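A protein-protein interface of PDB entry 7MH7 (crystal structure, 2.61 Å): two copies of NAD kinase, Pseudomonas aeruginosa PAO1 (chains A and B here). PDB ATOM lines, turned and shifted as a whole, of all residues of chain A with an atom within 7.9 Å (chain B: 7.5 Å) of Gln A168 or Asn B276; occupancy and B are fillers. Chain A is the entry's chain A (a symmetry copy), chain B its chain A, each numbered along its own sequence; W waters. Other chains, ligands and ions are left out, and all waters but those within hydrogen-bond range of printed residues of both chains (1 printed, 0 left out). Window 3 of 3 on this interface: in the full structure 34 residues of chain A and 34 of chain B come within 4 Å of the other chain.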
ATOM      1  N   LEU A 163      16.440  -1.085  36.351  1.00  0.00           N
ATOM      2  CA  LEU A 163      15.713  -1.285  35.106  1.00  0.00           C
ATOM      3  C   LEU A 163      16.526  -0.732  33.943  1.00  0.00           C
ATOM      4  O   LEU A 163      17.050   0.383  34.022  1.00  0.00           O
ATOM      5  CB  LEU A 163      14.337  -0.615  35.156  1.00  0.00           C
ATOM      6  CG  LEU A 163      13.487  -0.724  33.887  1.00  0.00           C
ATOM      7  CD1 LEU A 163      13.262  -2.183  33.519  1.00  0.00           C
ATOM      8  CD2 LEU A 163      12.161   0.004  34.057  1.00  0.00           C
ATOM      9  N   TYR A 164      16.629  -1.516  32.872  1.00  0.00           N
ATOM     10  CA  TYR A 164      17.313  -1.104  31.654  1.00  0.00           C
ATOM     11  C   TYR A 164      16.398  -1.354  30.465  1.00  0.00           C
ATOM     12  O   TYR A 164      15.838  -2.446  30.328  1.00  0.00           O
ATOM     13  CB  TYR A 164      18.635  -1.859  31.468  1.00  0.00           C
ATOM     14  CG  TYR A 164      19.710  -1.501  32.471  1.00  0.00           C
ATOM     15  CD1 TYR A 164      19.808  -2.170  33.683  1.00  0.00           C
ATOM     16  CD2 TYR A 164      20.633  -0.499  32.199  1.00  0.00           C
ATOM     17  CE1 TYR A 164      20.791  -1.848  34.599  1.00  0.00           C
ATOM     18  CE2 TYR A 164      21.619  -0.171  33.111  1.00  0.00           C
ATOM     19  CZ  TYR A 164      21.693  -0.849  34.308  1.00  0.00           C
ATOM     20  OH  TYR A 164      22.673  -0.525  35.217  1.00  0.00           O
ATOM     21  N   ILE A 165      16.248  -0.344  29.613  1.00  0.00           N
ATOM     22  CA  ILE A 165      15.453  -0.446  28.394  1.00  0.00           C
ATOM     23  C   ILE A 165      16.368  -0.142  27.217  1.00  0.00           C
ATOM     24  O   ILE A 165      16.885   0.978  27.101  1.00  0.00           O
ATOM     25  CB  ILE A 165      14.246   0.503  28.413  1.00  0.00           C
ATOM     26  CG1 ILE A 165      13.361   0.212  29.626  1.00  0.00           C
ATOM     27  CG2 ILE A 165      13.450   0.371  27.124  1.00  0.00           C
ATOM     28  CD1 ILE A 165      12.121   1.073  29.700  1.00  0.00           C
ATOM     29  N   ASP A 166      16.563  -1.135  26.348  1.00  0.00           N
ATOM     30  CA  ASP A 166      17.467  -1.020  25.202  1.00  0.00           C
ATOM     31  C   ASP A 166      18.874  -0.633  25.648  1.00  0.00           C
ATOM     32  O   ASP A 166      19.532   0.217  25.045  1.00  0.00           O
ATOM     33  CB  ASP A 166      16.925  -0.028  24.168  1.00  0.00           C
ATOM     34  CG  ASP A 166      15.658  -0.520  23.495  1.00  0.00           C
ATOM     35  OD1 ASP A 166      15.540  -1.743  23.274  1.00  0.00           O
ATOM     36  OD2 ASP A 166      14.781   0.315  23.185  1.00  0.00           O
ATOM     37  N   GLY A 167      19.338  -1.265  26.727  1.00  0.00           N
ATOM     38  CA  GLY A 167      20.647  -0.985  27.282  1.00  0.00           C
ATOM     39  C   GLY A 167      20.794   0.364  27.948  1.00  0.00           C
ATOM     40  O   GLY A 167      21.899   0.697  28.394  1.00  0.00           O
ATOM     41  N   GLN A 168      19.724   1.146  28.037  1.00  0.00           N
ATOM     42  CA  GLN A 168      19.765   2.488  28.601  1.00  0.00           C
ATOM     43  C   GLN A 168      19.219   2.453  30.023  1.00  0.00           C
ATOM     44  O   GLN A 168      18.118   1.945  30.258  1.00  0.00           O
ATOM     45  CB  GLN A 168      18.957   3.452  27.731  1.00  0.00           C
ATOM     46  CG  GLN A 168      19.088   4.918  28.093  1.00  0.00           C
ATOM     47  CD  GLN A 168      18.454   5.817  27.049  1.00  0.00           C
ATOM     48  OE1 GLN A 168      18.300   5.427  25.892  1.00  0.00           O
ATOM     49  NE2 GLN A 168      18.077   7.023  27.455  1.00  0.00           N
ATOM     50  N   PHE A 169      19.991   2.988  30.966  1.00  0.00           N
ATOM     51  CA  PHE A 169      19.607   2.929  32.370  1.00  0.00           C
ATOM     52  C   PHE A 169      18.411   3.835  32.638  1.00  0.00           C
ATOM     53  O   PHE A 169      18.416   5.016  32.275  1.00  0.00           O
ATOM     54  CB  PHE A 169      20.785   3.323  33.260  1.00  0.00           C
ATOM     55  CG  PHE A 169      20.436   3.431  34.718  1.00  0.00           C
ATOM     56  CD1 PHE A 169      20.206   2.295  35.479  1.00  0.00           C
ATOM     57  CD2 PHE A 169      20.344   4.670  35.330  1.00  0.00           C
ATOM     58  CE1 PHE A 169      19.885   2.396  36.821  1.00  0.00           C
ATOM     59  CE2 PHE A 169      20.024   4.777  36.672  1.00  0.00           C
ATOM     60  CZ  PHE A 169      19.796   3.639  37.417  1.00  0.00           C
ATOM     61  N   VAL A 170      17.386   3.275  33.278  1.00  0.00           N
ATOM     62  CA  VAL A 170      16.176   4.021  33.602  1.00  0.00           C
ATOM     63  C   VAL A 170      16.257   4.516  35.041  1.00  0.00           C
ATOM     64  O   VAL A 170      16.313   5.727  35.286  1.00  0.00           O
ATOM     65  CB  VAL A 170      14.916   3.165  33.377  1.00  0.00           C
ATOM     66  CG1 VAL A 170      13.664   3.970  33.689  1.00  0.00           C
ATOM     67  CG2 VAL A 170      14.879   2.645  31.949  1.00  0.00           C
ATOM     68  N   CYS A 171      16.270   3.591  35.998  1.00  0.00           N
ATOM     69  CA  CYS A 171      16.315   3.948  37.412  1.00  0.00           C
ATOM     70  C   CYS A 171      16.598   2.699  38.235  1.00  0.00           C
ATOM     71  O   CYS A 171      16.457   1.570  37.759  1.00  0.00           O
ATOM     72  CB  CYS A 171      15.005   4.601  37.869  1.00  0.00           C
ATOM     73  SG  CYS A 171      13.564   3.503  37.836  1.00  0.00           S
ATOM     74  N   GLU A 227      13.779  -3.967  24.498  1.00  0.00           N
ATOM     75  CA  GLU A 227      14.337  -5.070  25.271  1.00  0.00           C
ATOM     76  C   GLU A 227      14.540  -4.594  26.702  1.00  0.00           C
ATOM     77  O   GLU A 227      15.277  -3.631  26.940  1.00  0.00           O
ATOM     78  CB  GLU A 227      15.654  -5.559  24.672  1.00  0.00           C
ATOM     79  CG  GLU A 227      16.137  -6.876  25.261  1.00  0.00           C
ATOM     80  CD  GLU A 227      17.501  -7.286  24.744  1.00  0.00           C
ATOM     81  OE1 GLU A 227      18.457  -6.495  24.893  1.00  0.00           O
ATOM     82  OE2 GLU A 227      17.616  -8.397  24.186  1.00  0.00           O
ATOM     83  N   LYS A 229      15.724  -5.152  30.703  1.00  0.00           N
ATOM     84  CA  LYS A 229      16.782  -5.831  31.446  1.00  0.00           C
ATOM     85  C   LYS A 229      16.654  -5.433  32.910  1.00  0.00           C
ATOM     86  O   LYS A 229      16.939  -4.287  33.271  1.00  0.00           O
ATOM     87  CB  LYS A 229      18.161  -5.473  30.892  1.00  0.00           C
ATOM     88  CG  LYS A 229      19.187  -6.588  30.999  1.00  0.00           C
ATOM     89  CD  LYS A 229      20.415  -6.275  30.158  1.00  0.00           C
ATOM     90  CE  LYS A 229      20.047  -6.091  28.691  1.00  0.00           C
ATOM     91  NZ  LYS A 229      21.212  -5.658  27.868  1.00  0.00           N
ATOM     92  N   LEU B  97      16.285  20.716  34.660  1.00  0.00           N
ATOM     93  CA  LEU B  97      16.061  19.930  33.456  1.00  0.00           C
ATOM     94  C   LEU B  97      14.570  19.693  33.237  1.00  0.00           C
ATOM     95  O   LEU B  97      13.825  19.400  34.174  1.00  0.00           O
ATOM     96  CB  LEU B  97      16.799  18.594  33.556  1.00  0.00           C
ATOM     97  CG  LEU B  97      17.463  18.066  32.283  1.00  0.00           C
ATOM     98  CD1 LEU B  97      18.495  19.056  31.764  1.00  0.00           C
ATOM     99  CD2 LEU B  97      18.103  16.714  32.550  1.00  0.00           C
ATOM    100  N   GLY B  98      14.138  19.829  31.980  1.00  0.00           N
ATOM    101  CA  GLY B  98      12.746  19.669  31.629  1.00  0.00           C
ATOM    102  C   GLY B  98      12.567  18.645  30.522  1.00  0.00           C
ATOM    103  O   GLY B  98      13.525  18.224  29.869  1.00  0.00           O
ATOM    104  N   ASP B 102      16.218  21.590  27.243  1.00  0.00           N
ATOM    105  CA  ASP B 102      17.381  20.746  27.482  1.00  0.00           C
ATOM    106  C   ASP B 102      18.623  21.504  27.928  1.00  0.00           C
ATOM    107  O   ASP B 102      19.430  20.943  28.673  1.00  0.00           O
ATOM    108  CB  ASP B 102      17.719  19.946  26.212  1.00  0.00           C
ATOM    109  CG  ASP B 102      18.262  18.563  26.517  1.00  0.00           C
ATOM    110  OD1 ASP B 102      19.026  18.421  27.494  1.00  0.00           O
ATOM    111  OD2 ASP B 102      17.921  17.616  25.778  1.00  0.00           O
ATOM    112  N   ILE B 121      20.826  16.136  17.604  1.00  0.00           N
ATOM    113  CA  ILE B 121      19.823  15.121  17.308  1.00  0.00           C
ATOM    114  C   ILE B 121      18.540  15.823  16.893  1.00  0.00           C
ATOM    115  O   ILE B 121      18.143  16.820  17.506  1.00  0.00           O
ATOM    116  CB  ILE B 121      19.566  14.199  18.519  1.00  0.00           C
ATOM    117  CG1 ILE B 121      20.865  13.546  18.993  1.00  0.00           C
ATOM    118  CG2 ILE B 121      18.526  13.137  18.179  1.00  0.00           C
ATOM    119  CD1 ILE B 121      20.688  12.649  20.199  1.00  0.00           C
ATOM    120  N   HIS B 199       6.762   6.776  26.513  1.00  0.00           N
ATOM    121  CA  HIS B 199       8.045   7.115  25.917  1.00  0.00           C
ATOM    122  C   HIS B 199       7.828   7.911  24.631  1.00  0.00           C
ATOM    123  O   HIS B 199       6.859   7.663  23.904  1.00  0.00           O
ATOM    124  CB  HIS B 199       8.847   5.843  25.629  1.00  0.00           C
ATOM    125  CG  HIS B 199      10.293   6.089  25.327  1.00  0.00           C
ATOM    126  ND1 HIS B 199      10.750   6.391  24.063  1.00  0.00           N
ATOM    127  CD2 HIS B 199      11.386   6.069  26.127  1.00  0.00           C
ATOM    128  CE1 HIS B 199      12.061   6.550  24.096  1.00  0.00           C
ATOM    129  NE2 HIS B 199      12.472   6.360  25.336  1.00  0.00           N
ATOM    130  N   LYS B 201       9.217   7.710  21.826  1.00  0.00           N
ATOM    131  CA  LYS B 201       9.257   6.872  20.633  1.00  0.00           C
ATOM    132  C   LYS B 201       7.902   6.269  20.288  1.00  0.00           C
ATOM    133  O   LYS B 201       7.729   5.774  19.169  1.00  0.00           O
ATOM    134  CB  LYS B 201      10.266   5.733  20.806  1.00  0.00           C
ATOM    135  CG  LYS B 201      11.727   6.126  20.675  1.00  0.00           C
ATOM    136  CD  LYS B 201      12.591   4.875  20.573  1.00  0.00           C
ATOM    137  CE  LYS B 201      14.071   5.206  20.548  1.00  0.00           C
ATOM    138  NZ  LYS B 201      14.552   5.692  21.869  1.00  0.00           N
ATOM    139  N   HIS B 271      18.038  18.450  19.929  1.00  0.00           N
ATOM    140  CA  HIS B 271      18.696  18.118  21.179  1.00  0.00           C
ATOM    141  C   HIS B 271      20.194  18.000  20.954  1.00  0.00           C
ATOM    142  O   HIS B 271      20.635  17.665  19.850  1.00  0.00           O
ATOM    143  CB  HIS B 271      18.182  16.792  21.762  1.00  0.00           C
ATOM    144  CG  HIS B 271      16.704  16.757  21.992  1.00  0.00           C
ATOM    145  ND1 HIS B 271      16.074  17.557  22.920  1.00  0.00           N
ATOM    146  CD2 HIS B 271      15.734  16.000  21.428  1.00  0.00           C
ATOM    147  CE1 HIS B 271      14.777  17.303  22.911  1.00  0.00           C
ATOM    148  NE2 HIS B 271      14.545  16.362  22.014  1.00  0.00           N
ATOM    149  N   PRO B 272      20.998  18.275  21.975  1.00  0.00           N
ATOM    150  CA  PRO B 272      22.402  17.867  21.925  1.00  0.00           C
ATOM    151  C   PRO B 272      22.511  16.352  21.973  1.00  0.00           C
ATOM    152  O   PRO B 272      21.581  15.645  22.365  1.00  0.00           O
ATOM    153  CB  PRO B 272      23.012  18.508  23.177  1.00  0.00           C
ATOM    154  CG  PRO B 272      22.066  19.589  23.551  1.00  0.00           C
ATOM    155  CD  PRO B 272      20.708  19.097  23.160  1.00  0.00           C
ATOM    156  N   ILE B 273      23.677  15.855  21.556  1.00  0.00           N
ATOM    157  CA  ILE B 273      23.926  14.421  21.618  1.00  0.00           C
ATOM    158  C   ILE B 273      23.937  13.929  23.062  1.00  0.00           C
ATOM    159  O   ILE B 273      23.689  12.744  23.317  1.00  0.00           O
ATOM    160  CB  ILE B 273      25.240  14.093  20.880  1.00  0.00           C
ATOM    161  CG1 ILE B 273      25.176  14.627  19.447  1.00  0.00           C
ATOM    162  CG2 ILE B 273      25.508  12.594  20.864  1.00  0.00           C
ATOM    163  CD1 ILE B 273      26.325  14.180  18.572  1.00  0.00           C
ATOM    164  N   ASP B 274      24.182  14.824  24.021  1.00  0.00           N
ATOM    165  CA  ASP B 274      24.175  14.511  25.445  1.00  0.00           C
ATOM    166  C   ASP B 274      22.777  14.217  25.987  1.00  0.00           C
ATOM    167  O   ASP B 274      22.648  13.892  27.172  1.00  0.00           O
ATOM    168  CB  ASP B 274      24.804  15.674  26.217  1.00  0.00           C
ATOM    169  CG  ASP B 274      25.171  15.308  27.640  1.00  0.00           C
ATOM    170  OD1 ASP B 274      26.043  14.434  27.823  1.00  0.00           O
ATOM    171  OD2 ASP B 274      24.591  15.899  28.575  1.00  0.00           O
ATOM    172  N   HIS B 275      21.741  14.301  25.156  1.00  0.00           N
ATOM    173  CA  HIS B 275      20.371  14.166  25.636  1.00  0.00           C
ATOM    174  C   HIS B 275      20.073  12.733  26.067  1.00  0.00           C
ATOM    175  O   HIS B 275      20.414  11.775  25.367  1.00  0.00           O
ATOM    176  CB  HIS B 275      19.394  14.602  24.546  1.00  0.00           C
ATOM    177  CG  HIS B 275      17.957  14.370  24.892  1.00  0.00           C
ATOM    178  ND1 HIS B 275      17.266  15.169  25.776  1.00  0.00           N
ATOM    179  CD2 HIS B 275      17.080  13.427  24.471  1.00  0.00           C
ATOM    180  CE1 HIS B 275      16.025  14.730  25.885  1.00  0.00           C
ATOM    181  NE2 HIS B 275      15.886  13.674  25.104  1.00  0.00           N
ATOM    182  N   ASN B 276      19.429  12.595  27.226  1.00  0.00           N
ATOM    183  CA  ASN B 276      18.992  11.301  27.741  1.00  0.00           C
ATOM    184  C   ASN B 276      17.611  11.482  28.350  1.00  0.00           C
ATOM    185  O   ASN B 276      17.446  12.259  29.296  1.00  0.00           O
ATOM    186  CB  ASN B 276      19.979  10.749  28.776  1.00  0.00           C
ATOM    187  CG  ASN B 276      19.557   9.397  29.329  1.00  0.00           C
ATOM    188  OD1 ASN B 276      18.648   8.752  28.806  1.00  0.00           O
ATOM    189  ND2 ASN B 276      20.224   8.960  30.391  1.00  0.00           N
ATOM    190  N   TYR B 277      16.624  10.763  27.811  1.00  0.00           N
ATOM    191  CA  TYR B 277      15.245  10.948  28.252  1.00  0.00           C
ATOM    192  C   TYR B 277      15.036  10.448  29.676  1.00  0.00           C
ATOM    193  O   TYR B 277      14.351  11.099  30.473  1.00  0.00           O
ATOM    194  CB  TYR B 277      14.289  10.243  27.291  1.00  0.00           C
ATOM    195  CG  TYR B 277      12.868  10.151  27.802  1.00  0.00           C
ATOM    196  CD1 TYR B 277      12.030  11.259  27.783  1.00  0.00           C
ATOM    197  CD2 TYR B 277      12.365   8.957  28.301  1.00  0.00           C
ATOM    198  CE1 TYR B 277      10.731  11.178  28.249  1.00  0.00           C
ATOM    199  CE2 TYR B 277      11.067   8.868  28.769  1.00  0.00           C
ATOM    200  CZ  TYR B 277      10.255   9.981  28.741  1.00  0.00           C
ATOM    201  OH  TYR B 277       8.963   9.897  29.205  1.00  0.00           O
ATOM    202  N   TYR B 278      15.610   9.293  30.017  1.00  0.00           N
ATOM    203  CA  TYR B 278      15.409   8.739  31.350  1.00  0.00           C
ATOM    204  C   TYR B 278      16.145   9.527  32.425  1.00  0.00           C
ATOM    205  O   TYR B 278      15.776   9.440  33.601  1.00  0.00           O
ATOM    206  CB  TYR B 278      15.837   7.271  31.382  1.00  0.00           C
ATOM    207  CG  TYR B 278      15.022   6.393  30.459  1.00  0.00           C
ATOM    208  CD1 TYR B 278      13.681   6.139  30.716  1.00  0.00           C
ATOM    209  CD2 TYR B 278      15.594   5.818  29.332  1.00  0.00           C
ATOM    210  CE1 TYR B 278      12.930   5.340  29.874  1.00  0.00           C
ATOM    211  CE2 TYR B 278      14.850   5.015  28.485  1.00  0.00           C
ATOM    212  CZ  TYR B 278      13.521   4.779  28.761  1.00  0.00           C
ATOM    213  OH  TYR B 278      12.777   3.982  27.922  1.00  0.00           O
ATOM    214  N   GLU B 279      17.175  10.294  32.055  1.00  0.00           N
ATOM    215  CA  GLU B 279      17.801  11.187  33.023  1.00  0.00           C
ATOM    216  C   GLU B 279      16.884  12.353  33.369  1.00  0.00           C
ATOM    217  O   GLU B 279      16.896  12.833  34.509  1.00  0.00           O
ATOM    218  CB  GLU B 279      19.140  11.697  32.489  1.00  0.00           C
ATOM    219  CG  GLU B 279      19.910  12.570  33.472  1.00  0.00           C
ATOM    220  CD  GLU B 279      21.260  13.009  32.936  1.00  0.00           C
ATOM    221  OE1 GLU B 279      21.614  12.604  31.809  1.00  0.00           O
ATOM    222  OE2 GLU B 279      21.966  13.759  33.642  1.00  0.00           O
ATOM    223  N   ILE B 280      16.084  12.815  32.405  1.00  0.00           N
ATOM    224  CA  ILE B 280      15.086  13.841  32.695  1.00  0.00           C
ATOM    225  C   ILE B 280      14.065  13.315  33.696  1.00  0.00           C
ATOM    226  O   ILE B 280      13.662  14.025  34.625  1.00  0.00           O
ATOM    227  CB  ILE B 280      14.411  14.314  31.395  1.00  0.00           C
ATOM    228  CG1 ILE B 280      15.457  14.820  30.400  1.00  0.00           C
ATOM    229  CG2 ILE B 280      13.384  15.398  31.687  1.00  0.00           C
ATOM    230  CD1 ILE B 280      14.873  15.262  29.079  1.00  0.00           C
ATOM    231  N   CYS B 281      13.635  12.062  33.525  1.00  0.00           N
ATOM    232  CA  CYS B 281      12.675  11.476  34.454  1.00  0.00           C
ATOM    233  C   CYS B 281      13.269  11.342  35.850  1.00  0.00           C
ATOM    234  O   CYS B 281      12.578  11.570  36.850  1.00  0.00           O
ATOM    235  CB  CYS B 281      12.207  10.115  33.939  1.00  0.00           C
ATOM    236  SG  CYS B 281      11.388  10.156  32.327  1.00  0.00           S
ATOM    237  N   ARG B 282      14.551  10.980  35.939  1.00  0.00           N
ATOM    238  CA  ARG B 282      15.184  10.808  37.243  1.00  0.00           C
ATOM    239  C   ARG B 282      15.292  12.125  38.000  1.00  0.00           C
ATOM    240  O   ARG B 282      15.277  12.128  39.236  1.00  0.00           O
ATOM    241  CB  ARG B 282      16.568  10.178  37.082  1.00  0.00           C
ATOM    242  CG  ARG B 282      16.541   8.692  36.777  1.00  0.00           C
ATOM    243  CD  ARG B 282      17.929   8.081  36.894  1.00  0.00           C
ATOM    244  NE  ARG B 282      18.849   8.604  35.891  1.00  0.00           N
ATOM    245  CZ  ARG B 282      18.980   8.112  34.667  1.00  0.00           C
ATOM    246  NH1 ARG B 282      18.250   7.089  34.253  1.00  0.00           N
ATOM    247  NH2 ARG B 282      19.864   8.659  33.838  1.00  0.00           N
ATOM    248  N   ARG B 290      21.974   5.320  39.931  1.00  0.00           N
ATOM    249  CA  ARG B 290      22.641   4.029  39.854  1.00  0.00           C
ATOM    250  C   ARG B 290      22.903   3.472  41.247  1.00  0.00           C
ATOM    251  O   ARG B 290      23.256   4.206  42.174  1.00  0.00           O
ATOM    252  CB  ARG B 290      23.954   4.153  39.082  1.00  0.00           C
ATOM    253  CG  ARG B 290      24.050   3.252  37.858  1.00  0.00           C
ATOM    254  CD  ARG B 290      24.217   4.067  36.582  1.00  0.00           C
ATOM    255  NE  ARG B 290      24.394   3.217  35.410  1.00  0.00           N
ATOM    256  CZ  ARG B 290      24.547   3.668  34.172  1.00  0.00           C
ATOM    257  NH1 ARG B 290      24.546   4.964  33.904  1.00  0.00           N
ATOM    258  NH2 ARG B 290      24.705   2.798  33.179  1.00  0.00           N
HETATM  259  O   HOH W   1      17.283   9.239  25.201  1.00  0.00           O
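The guanidinium group of Arg B282 lies within hydrogen-bond range of the backbone carbonyl oxygen of Phe A169, at 2.9 Å.
NH1 of Arg B282 sits at hydrogen-bond distance from O of Val A170.
The side-chain amide nitrogen (NE2) of Gln A168 lies close to the side-chain amide oxygen (OD1) of Asn B276, at 2.3 Å.
The side-chain amide oxygen of Asn B276 sits at hydrogen-bond distance from the backbone NH of Tyr B278 (3.3 Å).
The guanidinium group (NH2) of Arg B282 lies close to the side-chain amide nitrogen (ND2) of Asn B276.
O of Tyr B278 sits close to NH1 of Arg B282.
The backbone NH of Val A170 sits at hydrogen-bond distance from the backbone carbonyl oxygen of Leu A163, at 3.0 Å.
Ile A165 touches Tyr B278.
NE2 of Gln A168 touches CD2 of Tyr B278, 3.3 Å away.
Phe A169 touches Tyr B278.
Phe A169 touches Arg B290 (CZ to N, 3.7 Å).
Val A170 touches Tyr B278.
Water W1 lies within hydrogen-bond range of the backbone NH (N) of Tyr B277 (3.1 Å) and the side-chain amide nitrogen (NE2) of Gln A168 (3.3 Å).
No position is printed for both chains.
Of the 8 pairs that touch across the chains among the printed residues, none has its exchanged pair printed and touching as well.
Gln A168 touches just these residues of chain B: Asn B276 (2.3 Å) and Tyr B278 (3.3 Å).
Of chain A, only Gln A168 comes within 4 Å of Asn B276.
Printed residues of chain B within 4 Å of Ile A165: Tyr B278.
Of the printed residues of chain A, Arg B290 touches Phe A169 (3.7 Å).
Printed residues of chain B within 4 Å of Phe A169: Tyr B278 (3.5 Å), Arg B282 (2.9 Å) and Arg B290 (3.7 Å).
Of the printed residues of chain A, Arg B282 touches Phe A169 (2.9 Å) and Val A170 (2.6 Å).
Leu B97 touches none of the printed residues of chain A.
The nearest residue of chain A that does not touch Asn B276 is Phe A169 (4.7 Å).
The nearest printed residue of chain A that does not touch Tyr B278 is Cys A171 (5.9 Å).
Of the 19 printed residues of chain B, 4 touch a printed residue of chain A.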
